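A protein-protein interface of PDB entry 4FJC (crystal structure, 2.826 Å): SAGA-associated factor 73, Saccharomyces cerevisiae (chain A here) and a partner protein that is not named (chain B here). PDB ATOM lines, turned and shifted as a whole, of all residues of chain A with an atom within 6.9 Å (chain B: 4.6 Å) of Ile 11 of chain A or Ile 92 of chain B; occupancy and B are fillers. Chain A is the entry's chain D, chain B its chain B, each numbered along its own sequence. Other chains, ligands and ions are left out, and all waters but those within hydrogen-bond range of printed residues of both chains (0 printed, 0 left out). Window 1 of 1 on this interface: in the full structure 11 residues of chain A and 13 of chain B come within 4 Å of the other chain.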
ATOM      1  N   ILE A   8     -36.315  -9.362  -6.300  1.00  0.00           N
ATOM      2  CA  ILE A   8     -35.536  -9.384  -5.066  1.00  0.00           C
ATOM      3  C   ILE A   8     -35.953 -10.467  -4.089  1.00  0.00           C
ATOM      4  O   ILE A   8     -37.073 -10.462  -3.605  1.00  0.00           O
ATOM      5  CB  ILE A   8     -35.630  -8.036  -4.340  1.00  0.00           C
ATOM      6  CG1 ILE A   8     -35.081  -6.913  -5.244  1.00  0.00           C
ATOM      7  CG2 ILE A   8     -34.887  -8.109  -3.009  1.00  0.00           C
ATOM      8  CD1 ILE A   8     -34.670  -5.642  -4.521  1.00  0.00           C
ATOM      9  N   LYS A   9     -35.005 -11.354  -3.769  1.00  0.00           N
ATOM     10  CA  LYS A   9     -35.205 -12.496  -2.860  1.00  0.00           C
ATOM     11  C   LYS A   9     -35.185 -12.073  -1.401  1.00  0.00           C
ATOM     12  O   LYS A   9     -35.904 -12.637  -0.579  1.00  0.00           O
ATOM     13  CB  LYS A   9     -34.112 -13.561  -3.082  1.00  0.00           C
ATOM     14  CG  LYS A   9     -34.472 -14.960  -2.551  1.00  0.00           C
ATOM     15  CD  LYS A   9     -33.277 -15.875  -2.194  1.00  0.00           C
ATOM     16  CE  LYS A   9     -32.902 -15.883  -0.704  1.00  0.00           C
ATOM     17  NZ  LYS A   9     -31.740 -14.994  -0.379  1.00  0.00           N
ATOM     18  N   GLY A  10     -34.334 -11.106  -1.073  1.00  0.00           N
ATOM     19  CA  GLY A  10     -34.288 -10.545   0.276  1.00  0.00           C
ATOM     20  C   GLY A  10     -32.989  -9.814   0.485  1.00  0.00           C
ATOM     21  O   GLY A  10     -32.198  -9.723  -0.443  1.00  0.00           O
ATOM     22  N   ILE A  11     -32.758  -9.299   1.692  1.00  0.00           N
ATOM     23  CA  ILE A  11     -31.497  -8.630   2.005  1.00  0.00           C
ATOM     24  C   ILE A  11     -30.421  -9.679   2.208  1.00  0.00           C
ATOM     25  O   ILE A  11     -30.678 -10.706   2.825  1.00  0.00           O
ATOM     26  CB  ILE A  11     -31.582  -7.800   3.304  1.00  0.00           C
ATOM     27  CG1 ILE A  11     -32.602  -6.665   3.171  1.00  0.00           C
ATOM     28  CG2 ILE A  11     -30.226  -7.198   3.653  1.00  0.00           C
ATOM     29  CD1 ILE A  11     -32.866  -5.922   4.463  1.00  0.00           C
ATOM     30  N   LYS A  12     -29.212  -9.426   1.719  1.00  0.00           N
ATOM     31  CA  LYS A  12     -28.102 -10.323   2.024  1.00  0.00           C
ATOM     32  C   LYS A  12     -28.114 -10.640   3.517  1.00  0.00           C
ATOM     33  O   LYS A  12     -28.314  -9.735   4.330  1.00  0.00           O
ATOM     34  CB  LYS A  12     -26.763  -9.705   1.655  1.00  0.00           C
ATOM     35  CG  LYS A  12     -26.454  -9.740   0.171  1.00  0.00           C
ATOM     36  CD  LYS A  12     -25.268  -8.838  -0.173  1.00  0.00           C
ATOM     37  CE  LYS A  12     -25.173  -8.589  -1.670  1.00  0.00           C
ATOM     38  NZ  LYS A  12     -25.318  -9.860  -2.440  1.00  0.00           N
ATOM     39  N   PRO A  13     -27.944 -11.933   3.881  1.00  0.00           N
ATOM     40  CA  PRO A  13     -27.827 -12.366   5.286  1.00  0.00           C
ATOM     41  C   PRO A  13     -26.731 -11.679   6.096  1.00  0.00           C
ATOM     42  O   PRO A  13     -26.983 -11.250   7.223  1.00  0.00           O
ATOM     43  CB  PRO A  13     -27.544 -13.859   5.157  1.00  0.00           C
ATOM     44  CG  PRO A  13     -28.301 -14.252   3.937  1.00  0.00           C
ATOM     45  CD  PRO A  13     -28.182 -13.088   2.986  1.00  0.00           C
ATOM     46  N   LYS A  14     -25.533 -11.552   5.542  1.00  0.00           N
ATOM     47  CA  LYS A  14     -24.451 -10.911   6.297  1.00  0.00           C
ATOM     48  C   LYS A  14     -24.741  -9.446   6.633  1.00  0.00           C
ATOM     49  O   LYS A  14     -24.328  -8.967   7.688  1.00  0.00           O
ATOM     50  CB  LYS A  14     -23.093 -11.049   5.593  1.00  0.00           C
ATOM     51  CG  LYS A  14     -23.002 -10.452   4.192  1.00  0.00           C
ATOM     52  CD  LYS A  14     -21.548 -10.252   3.775  1.00  0.00           C
ATOM     53  CE  LYS A  14     -20.735 -11.551   3.749  1.00  0.00           C
ATOM     54  NZ  LYS A  14     -19.279 -11.247   3.745  1.00  0.00           N
ATOM     55  N   VAL A  15     -25.449  -8.749   5.744  1.00  0.00           N
ATOM     56  CA  VAL A  15     -25.880  -7.371   6.004  1.00  0.00           C
ATOM     57  C   VAL A  15     -26.911  -7.338   7.131  1.00  0.00           C
ATOM     58  O   VAL A  15     -26.794  -6.510   8.037  1.00  0.00           O
ATOM     59  CB  VAL A  15     -26.485  -6.687   4.759  1.00  0.00           C
ATOM     60  CG1 VAL A  15     -27.152  -5.387   5.158  1.00  0.00           C
ATOM     61  CG2 VAL A  15     -25.426  -6.417   3.702  1.00  0.00           C
ATOM     62  N   ILE A  16     -27.893  -8.248   7.091  1.00  0.00           N
ATOM     63  CA  ILE A  16     -28.946  -8.302   8.119  1.00  0.00           C
ATOM     64  C   ILE A  16     -28.403  -8.378   9.537  1.00  0.00           C
ATOM     65  O   ILE A  16     -28.950  -7.750  10.451  1.00  0.00           O
ATOM     66  CB  ILE A  16     -29.904  -9.497   7.952  1.00  0.00           C
ATOM     67  CG1 ILE A  16     -30.861  -9.264   6.786  1.00  0.00           C
ATOM     68  CG2 ILE A  16     -30.726  -9.698   9.222  1.00  0.00           C
ATOM     69  CD1 ILE A  16     -31.955 -10.303   6.683  1.00  0.00           C
ATOM     70  N   TYR A  19     -26.046  -5.059  10.543  1.00  0.00           N
ATOM     71  CA  TYR A  19     -26.798  -3.842  10.868  1.00  0.00           C
ATOM     72  C   TYR A  19     -28.001  -4.127  11.762  1.00  0.00           C
ATOM     73  O   TYR A  19     -28.843  -3.246  11.982  1.00  0.00           O
ATOM     74  CB  TYR A  19     -27.234  -3.130   9.585  1.00  0.00           C
ATOM     75  CG  TYR A  19     -26.098  -2.428   8.868  1.00  0.00           C
ATOM     76  CD1 TYR A  19     -25.759  -1.117   9.178  1.00  0.00           C
ATOM     77  CD2 TYR A  19     -25.362  -3.073   7.885  1.00  0.00           C
ATOM     78  CE1 TYR A  19     -24.730  -0.468   8.525  1.00  0.00           C
ATOM     79  CE2 TYR A  19     -24.330  -2.429   7.235  1.00  0.00           C
ATOM     80  CZ  TYR A  19     -24.024  -1.129   7.560  1.00  0.00           C
ATOM     81  OH  TYR A  19     -23.007  -0.484   6.915  1.00  0.00           O
ATOM     82  N   LEU A  21     -30.762  -5.571  11.382  1.00  0.00           N
ATOM     83  CA  LEU A  21     -32.014  -5.147  10.775  1.00  0.00           C
ATOM     84  C   LEU A  21     -33.234  -5.979  11.215  1.00  0.00           C
ATOM     85  O   LEU A  21     -34.365  -5.661  10.839  1.00  0.00           O
ATOM     86  CB  LEU A  21     -31.863  -5.148   9.253  1.00  0.00           C
ATOM     87  CG  LEU A  21     -30.719  -4.293   8.691  1.00  0.00           C
ATOM     88  CD1 LEU A  21     -30.709  -4.318   7.181  1.00  0.00           C
ATOM     89  CD2 LEU A  21     -30.840  -2.866   9.178  1.00  0.00           C
ATOM     90  N   GLN B  11     -36.443  -2.183   6.201  1.00  0.00           N
ATOM     91  CA  GLN B  11     -35.123  -2.662   6.610  1.00  0.00           C
ATOM     92  C   GLN B  11     -34.051  -2.081   5.709  1.00  0.00           C
ATOM     93  O   GLN B  11     -33.010  -1.645   6.174  1.00  0.00           O
ATOM     94  CB  GLN B  11     -35.064  -4.185   6.595  1.00  0.00           C
ATOM     95  CG  GLN B  11     -35.916  -4.832   7.680  1.00  0.00           C
ATOM     96  CD  GLN B  11     -35.806  -6.341   7.694  1.00  0.00           C
ATOM     97  OE1 GLN B  11     -35.015  -6.936   6.953  1.00  0.00           O
ATOM     98  NE2 GLN B  11     -36.603  -6.972   8.540  1.00  0.00           N
ATOM     99  N   ILE B  12     -34.325  -2.056   4.414  1.00  0.00           N
ATOM    100  CA  ILE B  12     -33.427  -1.431   3.458  1.00  0.00           C
ATOM    101  C   ILE B  12     -33.205   0.039   3.753  1.00  0.00           C
ATOM    102  O   ILE B  12     -32.141   0.547   3.458  1.00  0.00           O
ATOM    103  CB  ILE B  12     -33.962  -1.556   2.022  1.00  0.00           C
ATOM    104  CG1 ILE B  12     -33.670  -2.961   1.481  1.00  0.00           C
ATOM    105  CG2 ILE B  12     -33.320  -0.513   1.124  1.00  0.00           C
ATOM    106  CD1 ILE B  12     -34.210  -3.239   0.094  1.00  0.00           C
ATOM    107  N   TYR B  15     -30.740   0.424   6.876  1.00  0.00           N
ATOM    108  CA  TYR B  15     -29.356   0.263   6.489  1.00  0.00           C
ATOM    109  C   TYR B  15     -28.828   1.505   5.781  1.00  0.00           C
ATOM    110  O   TYR B  15     -27.671   1.883   5.936  1.00  0.00           O
ATOM    111  CB  TYR B  15     -29.166  -0.947   5.569  1.00  0.00           C
ATOM    112  CG  TYR B  15     -27.960  -0.774   4.655  1.00  0.00           C
ATOM    113  CD1 TYR B  15     -26.652  -0.976   5.131  1.00  0.00           C
ATOM    114  CD2 TYR B  15     -28.117  -0.346   3.322  1.00  0.00           C
ATOM    115  CE1 TYR B  15     -25.545  -0.791   4.300  1.00  0.00           C
ATOM    116  CE2 TYR B  15     -27.011  -0.149   2.497  1.00  0.00           C
ATOM    117  CZ  TYR B  15     -25.733  -0.376   2.995  1.00  0.00           C
ATOM    118  OH  TYR B  15     -24.664  -0.160   2.181  1.00  0.00           O
ATOM    119  N   PHE B  88     -26.744   1.787  -4.591  1.00  0.00           N
ATOM    120  CA  PHE B  88     -26.689   1.431  -3.171  1.00  0.00           C
ATOM    121  C   PHE B  88     -27.442   0.123  -2.853  1.00  0.00           C
ATOM    122  O   PHE B  88     -26.974  -0.688  -2.072  1.00  0.00           O
ATOM    123  CB  PHE B  88     -27.236   2.567  -2.322  1.00  0.00           C
ATOM    124  CG  PHE B  88     -26.330   3.754  -2.215  1.00  0.00           C
ATOM    125  CD1 PHE B  88     -25.056   3.625  -1.696  1.00  0.00           C
ATOM    126  CD2 PHE B  88     -26.785   5.023  -2.555  1.00  0.00           C
ATOM    127  CE1 PHE B  88     -24.229   4.732  -1.570  1.00  0.00           C
ATOM    128  CE2 PHE B  88     -25.969   6.136  -2.426  1.00  0.00           C
ATOM    129  CZ  PHE B  88     -24.685   5.995  -1.939  1.00  0.00           C
ATOM    130  N   LEU B  89     -28.603  -0.088  -3.452  1.00  0.00           N
ATOM    131  CA  LEU B  89     -29.372  -1.290  -3.149  1.00  0.00           C
ATOM    132  C   LEU B  89     -28.643  -2.579  -3.536  1.00  0.00           C
ATOM    133  O   LEU B  89     -28.815  -3.606  -2.872  1.00  0.00           O
ATOM    134  CB  LEU B  89     -30.756  -1.258  -3.812  1.00  0.00           C
ATOM    135  CG  LEU B  89     -31.814  -0.330  -3.211  1.00  0.00           C
ATOM    136  CD1 LEU B  89     -33.170  -0.764  -3.715  1.00  0.00           C
ATOM    137  CD2 LEU B  89     -31.791  -0.367  -1.699  1.00  0.00           C
ATOM    138  N   GLU B  90     -27.832  -2.516  -4.594  1.00  0.00           N
ATOM    139  CA  GLU B  90     -27.090  -3.680  -5.096  1.00  0.00           C
ATOM    140  C   GLU B  90     -25.955  -4.177  -4.205  1.00  0.00           C
ATOM    141  O   GLU B  90     -25.674  -5.371  -4.164  1.00  0.00           O
ATOM    142  CB  GLU B  90     -26.529  -3.370  -6.469  1.00  0.00           C
ATOM    143  CG  GLU B  90     -27.601  -3.361  -7.533  1.00  0.00           C
ATOM    144  CD  GLU B  90     -27.098  -2.768  -8.819  1.00  0.00           C
ATOM    145  OE1 GLU B  90     -25.859  -2.777  -9.036  1.00  0.00           O
ATOM    146  OE2 GLU B  90     -27.950  -2.285  -9.600  1.00  0.00           O
ATOM    147  N   GLU B  91     -25.290  -3.278  -3.498  1.00  0.00           N
ATOM    148  CA  GLU B  91     -24.315  -3.715  -2.510  1.00  0.00           C
ATOM    149  C   GLU B  91     -24.951  -4.596  -1.413  1.00  0.00           C
ATOM    150  O   GLU B  91     -24.228  -5.355  -0.761  1.00  0.00           O
ATOM    151  CB  GLU B  91     -23.598  -2.514  -1.884  1.00  0.00           C
ATOM    152  CG  GLU B  91     -22.622  -1.812  -2.833  1.00  0.00           C
ATOM    153  CD  GLU B  91     -22.208  -0.421  -2.349  1.00  0.00           C
ATOM    154  OE1 GLU B  91     -23.100   0.372  -1.965  1.00  0.00           O
ATOM    155  OE2 GLU B  91     -20.989  -0.117  -2.368  1.00  0.00           O
ATOM    156  N   ILE B  92     -26.278  -4.528  -1.217  1.00  0.00           N
ATOM    157  CA  ILE B  92     -26.914  -5.254  -0.103  1.00  0.00           C
ATOM    158  C   ILE B  92     -28.046  -6.227  -0.421  1.00  0.00           C
ATOM    159  O   ILE B  92     -28.459  -6.991   0.443  1.00  0.00           O
ATOM    160  CB  ILE B  92     -27.424  -4.267   0.960  1.00  0.00           C
ATOM    161  CG1 ILE B  92     -28.617  -3.469   0.445  1.00  0.00           C
ATOM    162  CG2 ILE B  92     -26.303  -3.320   1.370  1.00  0.00           C
ATOM    163  CD1 ILE B  92     -29.287  -2.670   1.524  1.00  0.00           C
ATOM    164  N   VAL B  93     -28.569  -6.195  -1.634  1.00  0.00           N
ATOM    165  CA  VAL B  93     -29.748  -7.002  -1.985  1.00  0.00           C
ATOM    166  C   VAL B  93     -29.429  -8.040  -3.054  1.00  0.00           C
ATOM    167  O   VAL B  93     -28.891  -7.695  -4.118  1.00  0.00           O
ATOM    168  CB  VAL B  93     -30.906  -6.099  -2.459  1.00  0.00           C
ATOM    169  CG1 VAL B  93     -31.701  -6.747  -3.577  1.00  0.00           C
ATOM    170  CG2 VAL B  93     -31.808  -5.762  -1.283  1.00  0.00           C
ATOM    171  N   ASP B  94     -29.755  -9.305  -2.779  1.00  0.00           N
ATOM    172  CA  ASP B  94     -29.520 -10.363  -3.772  1.00  0.00           C
ATOM    173  C   ASP B  94     -30.812 -10.678  -4.551  1.00  0.00           C
ATOM    174  O   ASP B  94     -31.914 -10.651  -4.016  1.00  0.00           O
ATOM    175  CB  ASP B  94     -28.777 -11.611  -3.203  1.00  0.00           C
ATOM    176  CG  ASP B  94     -29.324 -12.085  -1.860  1.00  0.00           C
ATOM    177  OD1 ASP B  94     -30.436 -11.635  -1.494  1.00  0.00           O
ATOM    178  OD2 ASP B  94     -28.649 -12.901  -1.176  1.00  0.00           O
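The side-chain amide nitrogen of Gln 11 of chain B is in hydrogen-bond range of the backbone carbonyl oxygen of Leu 21 of chain A, at 3.5 Å. The backbone NH (N) of Lys 12 of chain A is in hydrogen-bond range of the backbone carbonyl oxygen (O) of Ile 92 of chain B (2.9 Å). NZ of Lys 9 of chain A is in salt-bridge range of OD1 of Asp 94 of chain B (3.8 Å). N of Asp 94 of chain B sits at hydrogen-bond distance from O of Gly 10 of chain A (3.4 Å).
The backbone NH (N) of Leu 21 of chain A sits at hydrogen-bond distance from the backbone carbonyl oxygen (O) of Ile 16 of chain A.
CG1 of Val 93 of chain B touches CD1 of Ile 8 of chain A, 3.3 Å away. CA of Ile 8 of chain A touches O of Asp 94 of chain B, at 3.98 Å. Gly 10 of chain A touches Val 93 of chain B (O to CA, 3.97 Å). CD1 of Ile 11 of chain A touches OE1 of Gln 11 of chain B (3.4 Å). Ile 11 of chain A touches Ile 92 of chain B. Glu 91 of chain B touches Lys 12 of chain A. Lys 12 of chain A touches Asp 94 of chain B. Val 15 of chain A touches Ile 92 of chain B (CG2 to CG2, 3.97 Å). CE2 of Tyr 19 of chain A touches CD1 of Tyr 15 of chain B, 3.5 Å away.
Ile 11 of chain A touches two residues of chain B. Of the printed residues of chain B, Lys 9 of chain A touches Asp 94 (3.2 Å). Of the printed residues of chain A, Gln 11 of chain B touches Ile 11 and Leu 21. Printed residues of chain B within 4 Å of Tyr 19 of chain A: Tyr 15 (3.5 Å). Of the printed residues of chain A, Glu 91 of chain B touches Lys 12. Of the printed residues of chain B, Gly 10 of chain A touches Val 93 (3.97 Å) and Asp 94 (2.8 Å). The nearest residue of chain A that does not touch Ile 92 of chain B is Gly 10 of chain A (4.7 Å).
Hydrophobic or aromatic side chains of chain B within 4 Å of the printed part of chain A: Tyr 15, Ile 92 and Val 93. Of the 11 printed residues of chain A, 8 touch a printed residue of chain B. Hydrophobic or aromatic side chains of chain A that line the printed part of chain B: Ile 8, Ile 11, Val 15, Tyr 19 and Leu 21.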
